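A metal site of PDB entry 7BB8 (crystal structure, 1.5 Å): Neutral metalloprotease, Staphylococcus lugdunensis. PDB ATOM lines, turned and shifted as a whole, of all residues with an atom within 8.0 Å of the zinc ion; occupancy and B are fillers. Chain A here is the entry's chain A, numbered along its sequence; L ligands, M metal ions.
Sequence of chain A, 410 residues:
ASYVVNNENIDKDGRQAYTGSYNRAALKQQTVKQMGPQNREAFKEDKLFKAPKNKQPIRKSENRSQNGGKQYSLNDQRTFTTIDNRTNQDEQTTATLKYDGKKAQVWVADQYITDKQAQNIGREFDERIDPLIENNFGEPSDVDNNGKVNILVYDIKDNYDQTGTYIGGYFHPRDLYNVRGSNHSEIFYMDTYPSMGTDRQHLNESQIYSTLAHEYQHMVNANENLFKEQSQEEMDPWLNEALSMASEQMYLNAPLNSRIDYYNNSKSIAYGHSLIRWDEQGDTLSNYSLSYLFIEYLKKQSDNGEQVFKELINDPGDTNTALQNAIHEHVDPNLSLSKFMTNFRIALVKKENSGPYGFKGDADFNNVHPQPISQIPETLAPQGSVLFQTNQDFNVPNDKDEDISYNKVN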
ATOM      1  N   GLY A 169      -5.696  17.891  13.248  1.00  0.00           N
ATOM      2  CA  GLY A 169      -5.557  17.029  14.405  1.00  0.00           C
ATOM      3  C   GLY A 169      -4.114  16.968  14.833  1.00  0.00           C
ATOM      4  O   GLY A 169      -3.198  17.358  14.095  1.00  0.00           O
ATOM      5  N   TYR A 170      -3.919  16.451  16.050  1.00  0.00           N
ATOM      6  CA  TYR A 170      -2.548  16.273  16.494  1.00  0.00           C
ATOM      7  C   TYR A 170      -2.497  15.363  17.712  1.00  0.00           C
ATOM      8  O   TYR A 170      -3.511  15.033  18.317  1.00  0.00           O
ATOM      9  CB  TYR A 170      -1.827  17.585  16.787  1.00  0.00           C
ATOM     10  CG  TYR A 170      -2.577  18.651  17.523  1.00  0.00           C
ATOM     11  CD1 TYR A 170      -3.121  18.433  18.765  1.00  0.00           C
ATOM     12  CD2 TYR A 170      -2.684  19.915  16.975  1.00  0.00           C
ATOM     13  CE1 TYR A 170      -3.827  19.460  19.424  1.00  0.00           C
ATOM     14  CE2 TYR A 170      -3.345  20.931  17.631  1.00  0.00           C
ATOM     15  CZ  TYR A 170      -3.913  20.698  18.837  1.00  0.00           C
ATOM     16  OH  TYR A 170      -4.545  21.758  19.460  1.00  0.00           O
ATOM     17  N   PHE A 171      -1.265  14.964  18.020  1.00  0.00           N
ATOM     18  CA  PHE A 171      -0.876  14.131  19.142  1.00  0.00           C
ATOM     19  C   PHE A 171       0.222  14.886  19.868  1.00  0.00           C
ATOM     20  O   PHE A 171       1.104  15.462  19.229  1.00  0.00           O
ATOM     21  CB  PHE A 171      -0.360  12.753  18.662  1.00  0.00           C
ATOM     22  CG  PHE A 171       0.434  12.018  19.696  1.00  0.00           C
ATOM     23  CD1 PHE A 171      -0.182  11.398  20.758  1.00  0.00           C
ATOM     24  CD2 PHE A 171       1.811  11.977  19.604  1.00  0.00           C
ATOM     25  CE1 PHE A 171       0.556  10.728  21.705  1.00  0.00           C
ATOM     26  CE2 PHE A 171       2.566  11.309  20.578  1.00  0.00           C
ATOM     27  CZ  PHE A 171       1.925  10.701  21.624  1.00  0.00           C
ATOM     28  N   THR A 211      -7.044  10.945   9.037  1.00  0.00           N
ATOM     29  CA  THR A 211      -6.296  11.644  10.073  1.00  0.00           C
ATOM     30  C   THR A 211      -6.264  10.841  11.373  1.00  0.00           C
ATOM     31  O   THR A 211      -5.280  10.939  12.131  1.00  0.00           O
ATOM     32  CB  THR A 211      -6.868  13.042  10.289  1.00  0.00           C
ATOM     33  OG1 THR A 211      -6.713  13.802   9.082  1.00  0.00           O
ATOM     34  CG2 THR A 211      -6.141  13.763  11.405  1.00  0.00           C
ATOM     35  N   HIS A 214      -3.286   8.784  10.880  1.00  0.00           N
ATOM     36  CA  HIS A 214      -2.105   9.642  10.977  1.00  0.00           C
ATOM     37  C   HIS A 214      -1.714   9.858  12.435  1.00  0.00           C
ATOM     38  O   HIS A 214      -0.549   9.675  12.796  1.00  0.00           O
ATOM     39  CB  HIS A 214      -2.387  10.968  10.288  1.00  0.00           C
ATOM     40  CG  HIS A 214      -1.217  11.893  10.240  1.00  0.00           C
ATOM     41  ND1 HIS A 214      -0.628  12.314   9.066  1.00  0.00           N
ATOM     42  CD2 HIS A 214      -0.507  12.486  11.235  1.00  0.00           C
ATOM     43  CE1 HIS A 214       0.366  13.144   9.335  1.00  0.00           C
ATOM     44  NE2 HIS A 214       0.485  13.231  10.650  1.00  0.00           N
ATOM     45  N   GLU A 215      -2.680  10.249  13.268  1.00  0.00           N
ATOM     46  CA  GLU A 215      -2.382  10.567  14.670  1.00  0.00           C
ATOM     47  C   GLU A 215      -2.084   9.306  15.469  1.00  0.00           C
ATOM     48  O   GLU A 215      -1.188   9.303  16.318  1.00  0.00           O
ATOM     49  CB  GLU A 215      -3.535  11.326  15.309  1.00  0.00           C
ATOM     50  CG  GLU A 215      -3.864  12.649  14.621  1.00  0.00           C
ATOM     51  CD  GLU A 215      -2.667  13.523  14.427  1.00  0.00           C
ATOM     52  OE1 GLU A 215      -1.696  13.446  15.231  1.00  0.00           O
ATOM     53  OE2 GLU A 215      -2.671  14.330  13.464  1.00  0.00           O
ATOM     54  N   GLN A 217      -0.649   6.620  14.419  1.00  0.00           N
ATOM     55  CA  GLN A 217       0.732   6.264  14.134  1.00  0.00           C
ATOM     56  C   GLN A 217       1.695   7.053  14.996  1.00  0.00           C
ATOM     57  O   GLN A 217       2.628   6.482  15.583  1.00  0.00           O
ATOM     58  CB  GLN A 217       1.033   6.460  12.657  1.00  0.00           C
ATOM     59  CG  GLN A 217       2.393   5.841  12.185  1.00  0.00           C
ATOM     60  CD  GLN A 217       3.685   6.462  12.714  1.00  0.00           C
ATOM     61  OE1 GLN A 217       4.636   5.734  13.083  1.00  0.00           O
ATOM     62  NE2 GLN A 217       3.752   7.812  12.730  1.00  0.00           N
ATOM     63  N   HIS A 218       1.462   8.369  15.137  1.00  0.00           N
ATOM     64  CA  HIS A 218       2.330   9.147  15.991  1.00  0.00           C
ATOM     65  C   HIS A 218       2.317   8.579  17.410  1.00  0.00           C
ATOM     66  O   HIS A 218       3.362   8.467  18.067  1.00  0.00           O
ATOM     67  CB  HIS A 218       1.912  10.614  16.032  1.00  0.00           C
ATOM     68  CG  HIS A 218       2.231  11.410  14.802  1.00  0.00           C
ATOM     69  ND1 HIS A 218       3.435  11.320  14.138  1.00  0.00           N
ATOM     70  CD2 HIS A 218       1.552  12.427  14.218  1.00  0.00           C
ATOM     71  CE1 HIS A 218       3.451  12.206  13.145  1.00  0.00           C
ATOM     72  NE2 HIS A 218       2.329  12.886  13.180  1.00  0.00           N
ATOM     73  N   PRO A 237      11.671  13.629  13.336  1.00  0.00           N
ATOM     74  CA  PRO A 237      10.330  14.007  12.862  1.00  0.00           C
ATOM     75  C   PRO A 237      10.073  13.743  11.391  1.00  0.00           C
ATOM     76  O   PRO A 237       8.973  13.317  11.054  1.00  0.00           O
ATOM     77  CB  PRO A 237      10.283  15.511  13.200  1.00  0.00           C
ATOM     78  CG  PRO A 237      11.060  15.585  14.499  1.00  0.00           C
ATOM     79  CD  PRO A 237      12.241  14.629  14.268  1.00  0.00           C
ATOM     80  N   ASN A 240       8.999  10.175  11.198  1.00  0.00           N
ATOM     81  CA  ASN A 240       7.770   9.951  11.947  1.00  0.00           C
ATOM     82  C   ASN A 240       6.575  10.451  11.135  1.00  0.00           C
ATOM     83  O   ASN A 240       5.591   9.733  10.949  1.00  0.00           O
ATOM     84  CB  ASN A 240       7.874  10.651  13.290  1.00  0.00           C
ATOM     85  CG  ASN A 240       6.843  10.188  14.276  1.00  0.00           C
ATOM     86  OD1 ASN A 240       5.722   9.744  13.927  1.00  0.00           O
ATOM     87  ND2 ASN A 240       7.174  10.320  15.579  1.00  0.00           N
ATOM     88  N   GLU A 241       6.686  11.647  10.561  1.00  0.00           N
ATOM     89  CA  GLU A 241       5.605  12.152   9.726  1.00  0.00           C
ATOM     90  C   GLU A 241       5.437  11.276   8.478  1.00  0.00           C
ATOM     91  O   GLU A 241       4.309  10.990   8.071  1.00  0.00           O
ATOM     92  CB  GLU A 241       5.892  13.613   9.317  1.00  0.00           C
ATOM     93  CG  GLU A 241       5.941  14.579  10.501  1.00  0.00           C
ATOM     94  CD  GLU A 241       4.600  14.729  11.196  1.00  0.00           C
ATOM     95  OE1 GLU A 241       3.531  14.241  10.676  1.00  0.00           O
ATOM     96  OE2 GLU A 241       4.557  15.347  12.312  1.00  0.00           O
ATOM     97  N   ALA A 242       6.547  10.869   7.868  1.00  0.00           N
ATOM     98  CA  ALA A 242       6.475   9.972   6.721  1.00  0.00           C
ATOM     99  C   ALA A 242       5.608   8.765   7.035  1.00  0.00           C
ATOM    100  O   ALA A 242       4.731   8.389   6.245  1.00  0.00           O
ATOM    101  CB  ALA A 242       7.870   9.551   6.297  1.00  0.00           C
ATOM    102  N   LEU A 243       5.874   8.114   8.172  1.00  0.00           N
ATOM    103  CA  LEU A 243       5.166   6.902   8.529  1.00  0.00           C
ATOM    104  C   LEU A 243       3.695   7.182   8.801  1.00  0.00           C
ATOM    105  O   LEU A 243       2.828   6.373   8.429  1.00  0.00           O
ATOM    106  CB  LEU A 243       5.834   6.254   9.730  1.00  0.00           C
ATOM    107  CG  LEU A 243       7.194   5.608   9.432  1.00  0.00           C
ATOM    108  CD1 LEU A 243       8.017   5.341  10.674  1.00  0.00           C
ATOM    109  CD2 LEU A 243       6.983   4.289   8.680  1.00  0.00           C
ATOM    110  N   SER A 244       3.378   8.349   9.397  1.00  0.00           N
ATOM    111  CA  SER A 244       1.978   8.715   9.549  1.00  0.00           C
ATOM    112  C   SER A 244       1.285   8.789   8.186  1.00  0.00           C
ATOM    113  O   SER A 244       0.168   8.276   8.015  1.00  0.00           O
ATOM    114  CB  SER A 244       1.839  10.040  10.302  1.00  0.00           C
ATOM    115  OG  SER A 244       1.934   9.809  11.672  1.00  0.00           O
ATOM    116  N   MET A 245       1.937   9.411   7.203  1.00  0.00           N
ATOM    117  CA  MET A 245       1.347   9.522   5.875  1.00  0.00           C
ATOM    118  C   MET A 245       1.291   8.169   5.163  1.00  0.00           C
ATOM    119  O   MET A 245       0.299   7.898   4.490  1.00  0.00           O
ATOM    120  CB  MET A 245       2.083  10.578   5.095  1.00  0.00           C
ATOM    121  CG  MET A 245       1.701  12.006   5.583  1.00  0.00           C
ATOM    122  SD  MET A 245       2.580  13.281   4.698  1.00  0.00           S
ATOM    123  CE  MET A 245       4.187  13.007   5.359  1.00  0.00           C
ATOM    124  N   GLU A 248      -1.871   6.656   6.305  1.00  0.00           N
ATOM    125  CA  GLU A 248      -3.029   7.231   5.626  1.00  0.00           C
ATOM    126  C   GLU A 248      -3.254   6.566   4.268  1.00  0.00           C
ATOM    127  O   GLU A 248      -4.396   6.247   3.908  1.00  0.00           O
ATOM    128  CB  GLU A 248      -2.866   8.739   5.415  1.00  0.00           C
ATOM    129  CG  GLU A 248      -2.849   9.491   6.698  1.00  0.00           C
ATOM    130  CD  GLU A 248      -2.918  10.973   6.479  1.00  0.00           C
ATOM    131  OE1 GLU A 248      -4.026  11.485   6.201  1.00  0.00           O
ATOM    132  OE2 GLU A 248      -1.858  11.640   6.540  1.00  0.00           O
ATOM    133  N   ARG A 259      -0.799  15.629  -1.545  1.00  0.00           N
ATOM    134  CA  ARG A 259       0.615  15.760  -1.218  1.00  0.00           C
ATOM    135  C   ARG A 259       1.454  15.822  -2.480  1.00  0.00           C
ATOM    136  O   ARG A 259       2.438  16.590  -2.550  1.00  0.00           O
ATOM    137  CB  ARG A 259       1.078  14.590  -0.348  1.00  0.00           C
ATOM    138  CG  ARG A 259       0.369  14.456   0.998  1.00  0.00           C
ATOM    139  CD  ARG A 259       0.755  15.589   1.922  1.00  0.00           C
ATOM    140  NE  ARG A 259       0.078  15.451   3.210  1.00  0.00           N
ATOM    141  CZ  ARG A 259      -0.029  16.429   4.098  1.00  0.00           C
ATOM    142  NH1 ARG A 259       0.493  17.640   3.862  1.00  0.00           N
ATOM    143  NH2 ARG A 259      -0.665  16.211   5.233  1.00  0.00           N
ATOM    144  N   TRP A 278      13.515  19.643   9.090  1.00  0.00           N
ATOM    145  CA  TRP A 278      12.103  19.940   9.156  1.00  0.00           C
ATOM    146  C   TRP A 278      11.914  21.463   9.325  1.00  0.00           C
ATOM    147  O   TRP A 278      12.316  22.041  10.345  1.00  0.00           O
ATOM    148  CB  TRP A 278      11.430  19.180  10.313  1.00  0.00           C
ATOM    149  CG  TRP A 278       9.966  19.214  10.221  1.00  0.00           C
ATOM    150  CD1 TRP A 278       9.138  20.085  10.853  1.00  0.00           C
ATOM    151  CD2 TRP A 278       9.128  18.337   9.459  1.00  0.00           C
ATOM    152  NE1 TRP A 278       7.830  19.821  10.524  1.00  0.00           N
ATOM    153  CE2 TRP A 278       7.809  18.746   9.655  1.00  0.00           C
ATOM    154  CE3 TRP A 278       9.378  17.239   8.619  1.00  0.00           C
ATOM    155  CZ2 TRP A 278       6.727  18.119   9.049  1.00  0.00           C
ATOM    156  CZ3 TRP A 278       8.301  16.609   8.037  1.00  0.00           C
ATOM    157  CH2 TRP A 278       6.997  17.052   8.239  1.00  0.00           C
ATOM    158  N   TYR A 288       6.145  17.736   4.457  1.00  0.00           N
ATOM    159  CA  TYR A 288       5.153  16.675   4.404  1.00  0.00           C
ATOM    160  C   TYR A 288       5.204  15.953   3.049  1.00  0.00           C
ATOM    161  O   TYR A 288       5.182  14.717   2.999  1.00  0.00           O
ATOM    162  CB  TYR A 288       3.755  17.206   4.672  1.00  0.00           C
ATOM    163  CG  TYR A 288       3.460  17.446   6.147  1.00  0.00           C
ATOM    164  CD1 TYR A 288       3.028  16.399   6.959  1.00  0.00           C
ATOM    165  CD2 TYR A 288       3.585  18.700   6.716  1.00  0.00           C
ATOM    166  CE1 TYR A 288       2.750  16.579   8.309  1.00  0.00           C
ATOM    167  CE2 TYR A 288       3.291  18.896   8.070  1.00  0.00           C
ATOM    168  CZ  TYR A 288       2.880  17.849   8.863  1.00  0.00           C
ATOM    169  OH  TYR A 288       2.600  18.046  10.189  1.00  0.00           O
HETATM  170 AS1  LIG L   1      -0.153  16.393  12.253  1.00  0.00          AS
HETATM  171  O1  LIG L   1       1.320  16.167  11.543  1.00  0.00           O
HETATM  172  O2  LIG L   1      -0.392  15.109  13.420  1.00  0.00           O
HETATM  173  C1  LIG L   1      -0.131  18.168  13.054  1.00  0.00           C
HETATM  174  C2  LIG L   1      -1.628  16.275  10.939  1.00  0.00           C
HETATM  175 ZN    ZN M   1       1.850  14.206  11.740  1.00  0.00          ZN
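OE1 of Glu 241 is bound to the zinc ion, 2.0 Å away. NE2 of His 214 is bound to the zinc ion, 2.0 Å away. NE2 of His 218 binds the zinc ion (2.0 Å). The zinc ion is bound by an oxygen (O1) of the ligand, 2.0 Å away. The zinc ion has four donor atoms within binding distance.
The nearest printed residue that does not touch the zinc ion is Tyr 288 (4.2 Å).
The backbone carbonyl oxygen (O) of His 214 is in hydrogen-bond range of the side-chain hydroxyl (OG) of Ser 244, 2.7 Å away. ND1 of His 214 sits at hydrogen-bond distance from OE2 of Glu 248, 2.9 Å away. The side-chain hydroxyl of Ser 244 lies close to a ring nitrogen (ND1) of His 218 (3.3 Å). The side-chain amide oxygen of Asn 240 sits at hydrogen-bond distance from a ring nitrogen (ND1) of His 218 (2.8 Å).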
